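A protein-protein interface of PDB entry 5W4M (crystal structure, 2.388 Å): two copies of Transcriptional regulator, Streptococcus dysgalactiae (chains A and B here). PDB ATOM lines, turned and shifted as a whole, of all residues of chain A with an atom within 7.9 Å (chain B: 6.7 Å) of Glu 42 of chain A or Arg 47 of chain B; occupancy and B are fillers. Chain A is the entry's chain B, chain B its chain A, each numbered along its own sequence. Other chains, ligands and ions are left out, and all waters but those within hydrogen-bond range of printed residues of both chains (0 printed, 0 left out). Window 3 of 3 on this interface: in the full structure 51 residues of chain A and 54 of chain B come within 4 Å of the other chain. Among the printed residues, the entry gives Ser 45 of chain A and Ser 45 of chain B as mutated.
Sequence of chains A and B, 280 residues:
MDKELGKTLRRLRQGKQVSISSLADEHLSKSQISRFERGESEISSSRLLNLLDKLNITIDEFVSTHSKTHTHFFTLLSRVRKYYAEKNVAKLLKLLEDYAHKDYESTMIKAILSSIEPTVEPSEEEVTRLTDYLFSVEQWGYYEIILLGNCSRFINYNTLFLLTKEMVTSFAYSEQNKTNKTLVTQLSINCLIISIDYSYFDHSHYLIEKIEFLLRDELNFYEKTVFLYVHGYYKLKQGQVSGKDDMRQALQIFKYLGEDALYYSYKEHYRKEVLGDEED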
ATOM      1  N   LYS A   3     -28.347 -28.721 -17.780  1.00  0.00           N
ATOM      2  CA  LYS A   3     -28.381 -29.899 -16.921  1.00  0.00           C
ATOM      3  C   LYS A   3     -27.163 -30.791 -17.170  1.00  0.00           C
ATOM      4  O   LYS A   3     -26.608 -31.372 -16.236  1.00  0.00           O
ATOM      5  CB  LYS A   3     -29.679 -30.683 -17.145  1.00  0.00           C
ATOM      6  CG  LYS A   3     -29.687 -32.086 -16.555  1.00  0.00           C
ATOM      7  CD  LYS A   3     -29.536 -32.068 -15.043  1.00  0.00           C
ATOM      8  CE  LYS A   3     -28.955 -33.380 -14.547  1.00  0.00           C
ATOM      9  NZ  LYS A   3     -29.592 -34.543 -15.226  1.00  0.00           N
ATOM     10  N   LEU A   5     -23.971 -30.252 -17.644  1.00  0.00           N
ATOM     11  CA  LEU A   5     -22.834 -29.344 -17.536  1.00  0.00           C
ATOM     12  C   LEU A   5     -21.547 -29.996 -18.024  1.00  0.00           C
ATOM     13  O   LEU A   5     -20.695 -29.321 -18.615  1.00  0.00           O
ATOM     14  CB  LEU A   5     -22.668 -28.876 -16.089  1.00  0.00           C
ATOM     15  CG  LEU A   5     -23.840 -28.161 -15.418  1.00  0.00           C
ATOM     16  CD1 LEU A   5     -23.460 -27.732 -14.012  1.00  0.00           C
ATOM     17  CD2 LEU A   5     -24.268 -26.962 -16.235  1.00  0.00           C
ATOM     18  N   GLY A   6     -21.392 -31.302 -17.795  1.00  0.00           N
ATOM     19  CA  GLY A   6     -20.156 -31.970 -18.160  1.00  0.00           C
ATOM     20  C   GLY A   6     -19.935 -32.065 -19.654  1.00  0.00           C
ATOM     21  O   GLY A   6     -18.789 -32.069 -20.113  1.00  0.00           O
ATOM     22  N   LEU A  28     -10.592 -33.910  -6.878  1.00  0.00           N
ATOM     23  CA  LEU A  28     -11.414 -34.573  -7.881  1.00  0.00           C
ATOM     24  C   LEU A  28     -10.537 -35.522  -8.680  1.00  0.00           C
ATOM     25  O   LEU A  28      -9.461 -35.132  -9.143  1.00  0.00           O
ATOM     26  CB  LEU A  28     -12.083 -33.551  -8.802  1.00  0.00           C
ATOM     27  CG  LEU A  28     -13.400 -33.966  -9.453  1.00  0.00           C
ATOM     28  CD1 LEU A  28     -14.436 -34.312  -8.397  1.00  0.00           C
ATOM     29  CD2 LEU A  28     -13.895 -32.847 -10.345  1.00  0.00           C
ATOM     30  N   GLN A  32     -13.934 -39.365 -11.479  1.00  0.00           N
ATOM     31  CA  GLN A  32     -14.992 -38.431 -11.111  1.00  0.00           C
ATOM     32  C   GLN A  32     -15.200 -37.380 -12.193  1.00  0.00           C
ATOM     33  O   GLN A  32     -16.340 -36.996 -12.482  1.00  0.00           O
ATOM     34  CB  GLN A  32     -14.668 -37.777  -9.769  1.00  0.00           C
ATOM     35  CG  GLN A  32     -14.757 -38.725  -8.583  1.00  0.00           C
ATOM     36  CD  GLN A  32     -14.226 -38.109  -7.303  1.00  0.00           C
ATOM     37  OE1 GLN A  32     -13.341 -37.253  -7.333  1.00  0.00           O
ATOM     38  NE2 GLN A  32     -14.764 -38.542  -6.169  1.00  0.00           N
ATOM     39  N   ARG A  35     -17.029 -39.179 -15.256  1.00  0.00           N
ATOM     40  CA  ARG A  35     -18.447 -39.433 -15.025  1.00  0.00           C
ATOM     41  C   ARG A  35     -19.265 -38.151 -15.134  1.00  0.00           C
ATOM     42  O   ARG A  35     -20.394 -38.167 -15.637  1.00  0.00           O
ATOM     43  CB  ARG A  35     -18.643 -40.090 -13.658  1.00  0.00           C
ATOM     44  CG  ARG A  35     -20.097 -40.335 -13.276  1.00  0.00           C
ATOM     45  CD  ARG A  35     -20.224 -41.371 -12.166  1.00  0.00           C
ATOM     46  NE  ARG A  35     -19.343 -41.091 -11.035  1.00  0.00           N
ATOM     47  CZ  ARG A  35     -18.215 -41.750 -10.783  1.00  0.00           C
ATOM     48  NH1 ARG A  35     -17.823 -42.731 -11.585  1.00  0.00           N
ATOM     49  NH2 ARG A  35     -17.476 -41.424  -9.730  1.00  0.00           N
ATOM     50  N   PHE A  36     -18.708 -37.027 -14.679  1.00  0.00           N
ATOM     51  CA  PHE A  36     -19.416 -35.759 -14.814  1.00  0.00           C
ATOM     52  C   PHE A  36     -19.495 -35.321 -16.274  1.00  0.00           C
ATOM     53  O   PHE A  36     -20.541 -34.835 -16.723  1.00  0.00           O
ATOM     54  CB  PHE A  36     -18.739 -34.686 -13.960  1.00  0.00           C
ATOM     55  CG  PHE A  36     -19.190 -33.287 -14.275  1.00  0.00           C
ATOM     56  CD1 PHE A  36     -20.519 -32.924 -14.137  1.00  0.00           C
ATOM     57  CD2 PHE A  36     -18.282 -32.333 -14.704  1.00  0.00           C
ATOM     58  CE1 PHE A  36     -20.935 -31.638 -14.431  1.00  0.00           C
ATOM     59  CE2 PHE A  36     -18.691 -31.044 -14.996  1.00  0.00           C
ATOM     60  CZ  PHE A  36     -20.017 -30.697 -14.857  1.00  0.00           C
ATOM     61  N   GLY A  39     -22.268 -36.755 -18.297  1.00  0.00           N
ATOM     62  CA  GLY A  39     -23.611 -36.457 -17.844  1.00  0.00           C
ATOM     63  C   GLY A  39     -24.200 -37.474 -16.895  1.00  0.00           C
ATOM     64  O   GLY A  39     -25.420 -37.511 -16.723  1.00  0.00           O
ATOM     65  N   GLU A  40     -23.366 -38.303 -16.270  1.00  0.00           N
ATOM     66  CA  GLU A  40     -23.840 -39.359 -15.388  1.00  0.00           C
ATOM     67  C   GLU A  40     -23.879 -38.948 -13.923  1.00  0.00           C
ATOM     68  O   GLU A  40     -24.339 -39.736 -13.091  1.00  0.00           O
ATOM     69  CB  GLU A  40     -22.957 -40.602 -15.528  1.00  0.00           C
ATOM     70  CG  GLU A  40     -22.843 -41.133 -16.941  1.00  0.00           C
ATOM     71  CD  GLU A  40     -21.873 -42.291 -17.039  1.00  0.00           C
ATOM     72  OE1 GLU A  40     -21.400 -42.760 -15.983  1.00  0.00           O
ATOM     73  OE2 GLU A  40     -21.584 -42.730 -18.172  1.00  0.00           O
ATOM     74  N   SER A  41     -23.405 -37.752 -13.585  1.00  0.00           N
ATOM     75  CA  SER A  41     -23.388 -37.321 -12.195  1.00  0.00           C
ATOM     76  C   SER A  41     -23.293 -35.805 -12.139  1.00  0.00           C
ATOM     77  O   SER A  41     -22.889 -35.152 -13.105  1.00  0.00           O
ATOM     78  CB  SER A  41     -22.225 -37.953 -11.422  1.00  0.00           C
ATOM     79  OG  SER A  41     -20.983 -37.393 -11.816  1.00  0.00           O
ATOM     80  N   GLU A  42     -23.676 -35.259 -10.990  1.00  0.00           N
ATOM     81  CA  GLU A  42     -23.514 -33.848 -10.681  1.00  0.00           C
ATOM     82  C   GLU A  42     -22.230 -33.644  -9.883  1.00  0.00           C
ATOM     83  O   GLU A  42     -21.595 -34.596  -9.421  1.00  0.00           O
ATOM     84  CB  GLU A  42     -24.725 -33.327  -9.902  1.00  0.00           C
ATOM     85  CG  GLU A  42     -26.004 -33.235 -10.725  1.00  0.00           C
ATOM     86  CD  GLU A  42     -27.189 -32.734  -9.917  1.00  0.00           C
ATOM     87  OE1 GLU A  42     -27.164 -32.867  -8.674  1.00  0.00           O
ATOM     88  OE2 GLU A  42     -28.149 -32.211 -10.523  1.00  0.00           O
ATOM     89  N   ILE A  43     -21.849 -32.378  -9.720  1.00  0.00           N
ATOM     90  CA  ILE A  43     -20.608 -32.016  -9.043  1.00  0.00           C
ATOM     91  C   ILE A  43     -20.849 -30.752  -8.226  1.00  0.00           C
ATOM     92  O   ILE A  43     -21.647 -29.889  -8.607  1.00  0.00           O
ATOM     93  CB  ILE A  43     -19.453 -31.818 -10.054  1.00  0.00           C
ATOM     94  CG1 ILE A  43     -18.205 -31.233  -9.387  1.00  0.00           C
ATOM     95  CG2 ILE A  43     -19.893 -30.913 -11.192  1.00  0.00           C
ATOM     96  CD1 ILE A  43     -17.027 -31.139 -10.328  1.00  0.00           C
ATOM     97  N   SER A  44     -20.163 -30.655  -7.089  1.00  0.00           N
ATOM     98  CA  SER A  44     -20.335 -29.517  -6.200  1.00  0.00           C
ATOM     99  C   SER A  44     -19.827 -28.226  -6.844  1.00  0.00           C
ATOM    100  O   SER A  44     -18.982 -28.229  -7.746  1.00  0.00           O
ATOM    101  CB  SER A  44     -19.611 -29.764  -4.880  1.00  0.00           C
ATOM    102  OG  SER A  44     -18.220 -29.517  -5.002  1.00  0.00           O
ATOM    103  N   SER A  45     -20.355 -27.104  -6.349  1.00  0.00           N
ATOM    104  CA  SER A  45     -19.999 -25.804  -6.907  1.00  0.00           C
ATOM    105  C   SER A  45     -18.517 -25.510  -6.734  1.00  0.00           C
ATOM    106  O   SER A  45     -17.867 -24.992  -7.651  1.00  0.00           O
ATOM    107  CB  SER A  45     -20.835 -24.708  -6.251  1.00  0.00           C
ATOM    108  OG  SER A  45     -22.217 -24.970  -6.394  1.00  0.00           O
ATOM    109  N   HIS B  27     -37.776 -28.748  -3.472  1.00  0.00           N
ATOM    110  CA  HIS B  27     -36.661 -29.461  -4.089  1.00  0.00           C
ATOM    111  C   HIS B  27     -35.291 -29.072  -3.557  1.00  0.00           C
ATOM    112  O   HIS B  27     -34.304 -29.708  -3.942  1.00  0.00           O
ATOM    113  CB  HIS B  27     -36.689 -29.266  -5.613  1.00  0.00           C
ATOM    114  CG  HIS B  27     -38.067 -29.312  -6.191  1.00  0.00           C
ATOM    115  ND1 HIS B  27     -38.736 -30.496  -6.416  1.00  0.00           N
ATOM    116  CD2 HIS B  27     -38.912 -28.324  -6.568  1.00  0.00           C
ATOM    117  CE1 HIS B  27     -39.932 -30.235  -6.913  1.00  0.00           C
ATOM    118  NE2 HIS B  27     -40.064 -28.925  -7.016  1.00  0.00           N
ATOM    119  N   LEU B  28     -35.186 -28.063  -2.698  1.00  0.00           N
ATOM    120  CA  LEU B  28     -33.951 -27.766  -1.983  1.00  0.00           C
ATOM    121  C   LEU B  28     -34.326 -27.291  -0.590  1.00  0.00           C
ATOM    122  O   LEU B  28     -34.977 -26.253  -0.443  1.00  0.00           O
ATOM    123  CB  LEU B  28     -33.110 -26.721  -2.719  1.00  0.00           C
ATOM    124  CG  LEU B  28     -31.938 -26.143  -1.932  1.00  0.00           C
ATOM    125  CD1 LEU B  28     -30.678 -26.961  -2.132  1.00  0.00           C
ATOM    126  CD2 LEU B  28     -31.713 -24.715  -2.383  1.00  0.00           C
ATOM    127  N   GLN B  32     -30.392 -28.091   3.879  1.00  0.00           N
ATOM    128  CA  GLN B  32     -29.333 -28.131   2.875  1.00  0.00           C
ATOM    129  C   GLN B  32     -28.737 -26.747   2.645  1.00  0.00           C
ATOM    130  O   GLN B  32     -27.515 -26.605   2.528  1.00  0.00           O
ATOM    131  CB  GLN B  32     -29.867 -28.726   1.571  1.00  0.00           C
ATOM    132  CG  GLN B  32     -30.079 -30.235   1.643  1.00  0.00           C
ATOM    133  CD  GLN B  32     -30.803 -30.791   0.429  1.00  0.00           C
ATOM    134  OE1 GLN B  32     -31.477 -30.059  -0.296  1.00  0.00           O
ATOM    135  NE2 GLN B  32     -30.669 -32.095   0.206  1.00  0.00           N
ATOM    136  N   ILE B  43     -22.881 -28.105  -2.071  1.00  0.00           N
ATOM    137  CA  ILE B  43     -24.094 -27.996  -2.865  1.00  0.00           C
ATOM    138  C   ILE B  43     -23.712 -28.059  -4.337  1.00  0.00           C
ATOM    139  O   ILE B  43     -22.615 -27.651  -4.733  1.00  0.00           O
ATOM    140  CB  ILE B  43     -24.877 -26.702  -2.533  1.00  0.00           C
ATOM    141  CG1 ILE B  43     -26.360 -26.875  -2.854  1.00  0.00           C
ATOM    142  CG2 ILE B  43     -24.301 -25.500  -3.266  1.00  0.00           C
ATOM    143  CD1 ILE B  43     -27.209 -25.699  -2.430  1.00  0.00           C
ATOM    144  N   SER B  44     -24.614 -28.603  -5.148  1.00  0.00           N
ATOM    145  CA  SER B  44     -24.325 -28.778  -6.561  1.00  0.00           C
ATOM    146  C   SER B  44     -24.356 -27.438  -7.290  1.00  0.00           C
ATOM    147  O   SER B  44     -24.953 -26.459  -6.833  1.00  0.00           O
ATOM    148  CB  SER B  44     -25.323 -29.741  -7.204  1.00  0.00           C
ATOM    149  OG  SER B  44     -26.627 -29.188  -7.218  1.00  0.00           O
ATOM    150  N   SER B  45     -23.698 -27.411  -8.450  1.00  0.00           N
ATOM    151  CA  SER B  45     -23.639 -26.190  -9.244  1.00  0.00           C
ATOM    152  C   SER B  45     -25.030 -25.727  -9.657  1.00  0.00           C
ATOM    153  O   SER B  45     -25.350 -24.536  -9.560  1.00  0.00           O
ATOM    154  CB  SER B  45     -22.764 -26.417 -10.475  1.00  0.00           C
ATOM    155  OG  SER B  45     -21.541 -27.036 -10.112  1.00  0.00           O
ATOM    156  N   SER B  46     -25.871 -26.654 -10.122  1.00  0.00           N
ATOM    157  CA  SER B  46     -27.215 -26.273 -10.538  1.00  0.00           C
ATOM    158  C   SER B  46     -28.030 -25.747  -9.365  1.00  0.00           C
ATOM    159  O   SER B  46     -28.837 -24.828  -9.534  1.00  0.00           O
ATOM    160  CB  SER B  46     -27.924 -27.459 -11.199  1.00  0.00           C
ATOM    161  OG  SER B  46     -28.051 -28.549 -10.304  1.00  0.00           O
ATOM    162  N   ARG B  47     -27.822 -26.299  -8.167  1.00  0.00           N
ATOM    163  CA  ARG B  47     -28.561 -25.831  -7.000  1.00  0.00           C
ATOM    164  C   ARG B  47     -28.081 -24.460  -6.543  1.00  0.00           C
ATOM    165  O   ARG B  47     -28.882 -23.655  -6.050  1.00  0.00           O
ATOM    166  CB  ARG B  47     -28.438 -26.842  -5.860  1.00  0.00           C
ATOM    167  CG  ARG B  47     -29.662 -27.723  -5.673  1.00  0.00           C
ATOM    168  CD  ARG B  47     -29.267 -29.135  -5.268  1.00  0.00           C
ATOM    169  NE  ARG B  47     -29.436 -30.085  -6.364  1.00  0.00           N
ATOM    170  CZ  ARG B  47     -28.852 -31.277  -6.418  1.00  0.00           C
ATOM    171  NH1 ARG B  47     -28.055 -31.674  -5.435  1.00  0.00           N
ATOM    172  NH2 ARG B  47     -29.067 -32.073  -7.455  1.00  0.00           N
ATOM    173  N   LEU B  48     -26.786 -24.175  -6.690  1.00  0.00           N
ATOM    174  CA  LEU B  48     -26.291 -22.847  -6.346  1.00  0.00           C
ATOM    175  C   LEU B  48     -26.834 -21.799  -7.308  1.00  0.00           C
ATOM    176  O   LEU B  48     -27.260 -20.719  -6.883  1.00  0.00           O
ATOM    177  CB  LEU B  48     -24.763 -22.835  -6.345  1.00  0.00           C
ATOM    178  CG  LEU B  48     -24.127 -21.456  -6.157  1.00  0.00           C
ATOM    179  CD1 LEU B  48     -24.512 -20.870  -4.800  1.00  0.00           C
ATOM    180  CD2 LEU B  48     -22.621 -21.539  -6.303  1.00  0.00           C
ATOM    181  N   LEU B  49     -26.838 -22.108  -8.606  1.00  0.00           N
ATOM    182  CA  LEU B  49     -27.382 -21.179  -9.590  1.00  0.00           C
ATOM    183  C   LEU B  49     -28.865 -20.924  -9.360  1.00  0.00           C
ATOM    184  O   LEU B  49     -29.344 -19.808  -9.586  1.00  0.00           O
ATOM    185  CB  LEU B  49     -27.144 -21.714 -11.002  1.00  0.00           C
ATOM    186  CG  LEU B  49     -25.683 -21.785 -11.450  1.00  0.00           C
ATOM    187  CD1 LEU B  49     -25.568 -22.512 -12.782  1.00  0.00           C
ATOM    188  CD2 LEU B  49     -25.080 -20.389 -11.540  1.00  0.00           C
ATOM    189  N   ASN B  50     -29.605 -21.940  -8.912  1.00  0.00           N
ATOM    190  CA  ASN B  50     -31.021 -21.748  -8.619  1.00  0.00           C
ATOM    191  C   ASN B  50     -31.215 -20.809  -7.435  1.00  0.00           C
ATOM    192  O   ASN B  50     -32.119 -19.965  -7.448  1.00  0.00           O
ATOM    193  CB  ASN B  50     -31.685 -23.099  -8.355  1.00  0.00           C
ATOM    194  CG  ASN B  50     -33.103 -22.960  -7.839  1.00  0.00           C
ATOM    195  OD1 ASN B  50     -33.367 -23.167  -6.652  1.00  0.00           O
ATOM    196  ND2 ASN B  50     -34.025 -22.603  -8.728  1.00  0.00           N
ATOM    197  N   LEU B  51     -30.374 -20.942  -6.406  1.00  0.00           N
ATOM    198  CA  LEU B  51     -30.434 -20.034  -5.264  1.00  0.00           C
ATOM    199  C   LEU B  51     -30.184 -18.595  -5.694  1.00  0.00           C
ATOM    200  O   LEU B  51     -30.928 -17.682  -5.316  1.00  0.00           O
ATOM    201  CB  LEU B  51     -29.411 -20.454  -4.208  1.00  0.00           C
ATOM    202  CG  LEU B  51     -29.780 -21.617  -3.295  1.00  0.00           C
ATOM    203  CD1 LEU B  51     -28.566 -22.046  -2.483  1.00  0.00           C
ATOM    204  CD2 LEU B  51     -30.927 -21.215  -2.385  1.00  0.00           C
ATOM    205  N   LEU B  52     -29.125 -18.374  -6.481  1.00  0.00           N
ATOM    206  CA  LEU B  52     -28.786 -17.021  -6.908  1.00  0.00           C
ATOM    207  C   LEU B  52     -29.865 -16.431  -7.801  1.00  0.00           C
ATOM    208  O   LEU B  52     -30.111 -15.220  -7.761  1.00  0.00           O
ATOM    209  CB  LEU B  52     -27.436 -17.022  -7.627  1.00  0.00           C
ATOM    210  CG  LEU B  52     -26.260 -17.535  -6.794  1.00  0.00           C
ATOM    211  CD1 LEU B  52     -25.000 -17.611  -7.634  1.00  0.00           C
ATOM    212  CD2 LEU B  52     -26.038 -16.647  -5.575  1.00  0.00           C
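Ser 45 of chain B touches Leu 5 of chain A.
CB of Ser 44 of chain B touches OE1 of Glu 42 of chain A, at 3.9 Å.
Glu 42 of chain A touches Ser 46 of chain B (OE2 to OG, 3.7 Å).
O of Ile 43 of chain A touches CA of Ser 44 of chain B, at 3.5 Å.
Ser 44 of chain A touches Ile 43 of chain B.
O of Ser 44 of chain A touches OG of Ser 45 of chain B (3.7 Å).
Ser 45 of chain A touches Ser 45 of chain B (OG to CA, 3.4 Å).
CB of Leu 48 of chain B touches OG of Ser 45 of chain A (3.3 Å).
Ile 43 of chain A touches Ser 44 of chain B, and with the chains exchanged Ser 44 of chain A touches Ile 43 of chain B.
Ile 43 of chain A touches Ser 45 of chain B, and with the chains exchanged Ser 45 of chain A touches Ile 43 of chain B.
Ser 44 of chain A touches Ser 45 of chain B, and with the chains exchanged Ser 45 of chain A touches Ser 44 of chain B.
Ser 45 of chain A touches its own counterpart, Ser 45 of chain B.
5 positions are printed for both chains.
The backbone carbonyl oxygen of Ile 43 of chain B sits at hydrogen-bond distance from the backbone NH of Ser 45 of chain A, at 2.8 Å.
The backbone carbonyl oxygen (O) of Ser 44 of chain B is in hydrogen-bond range of the side-chain hydroxyl (OG) of Ser 45 of chain A (3.1 Å).
O of Ile 43 of chain A sits at hydrogen-bond distance from N of Ser 45 of chain B (3.2 Å).
The guanidinium group (NH2) of Arg 47 of chain B is in salt-bridge range of the side-chain carboxylate (OE2) of Glu 42 of chain A (3.2 Å).
Gly 39 of chain A touches none of the printed residues of chain B.
Glu 40 of chain A touches none of the printed residues of chain B.
Printed residues of chain B within 4 Å of Glu 42 of chain A: Ser 44, Ser 46 and Arg 47.
Of the printed residues of chain A, Ile 43 of chain B touches Ser 44 (3.3 Å) and Ser 45 (2.8 Å).
Of the printed residues of chain A, Leu 48 of chain B touches Ser 45 (3.3 Å).
The nearest printed residue of chain A that does not touch Ser 44 of chain B is Ser 44 of chain A (4.1 Å).
Of the 14 printed residues of chain A, 5 touch a printed residue of chain B.
Printed residues of chain A that touch a printed residue of chain B: Leu 5, Glu 42, Ile 43, Ser 44 and Ser 45.
Hydrophobic or aromatic side chains of chain A that line the printed part of chain B: Leu 5.
Along chain A the printed residues that touch a printed residue of chain B span positions 5 to 45.
Of the 13 printed residues of chain B, 6 touch a printed residue of chain A.
Hydrophobic or aromatic side chains of chain B that line the printed part of chain A: Ile 43 and Leu 48.
Among the printed residues, Asp or Glu carboxylates within 4 Å of a Lys or Arg side-chain nitrogen of the other chain: Glu 42 of chain A with Arg 47 of chain B.
OG of Ser 44 of chain B is in hydrogen-bond range of NE of Arg 47 of chain B (3.1 Å).
OG of Ser 44 of chain B sits at hydrogen-bond distance from OG of Ser 46 of chain B (3.5 Å).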
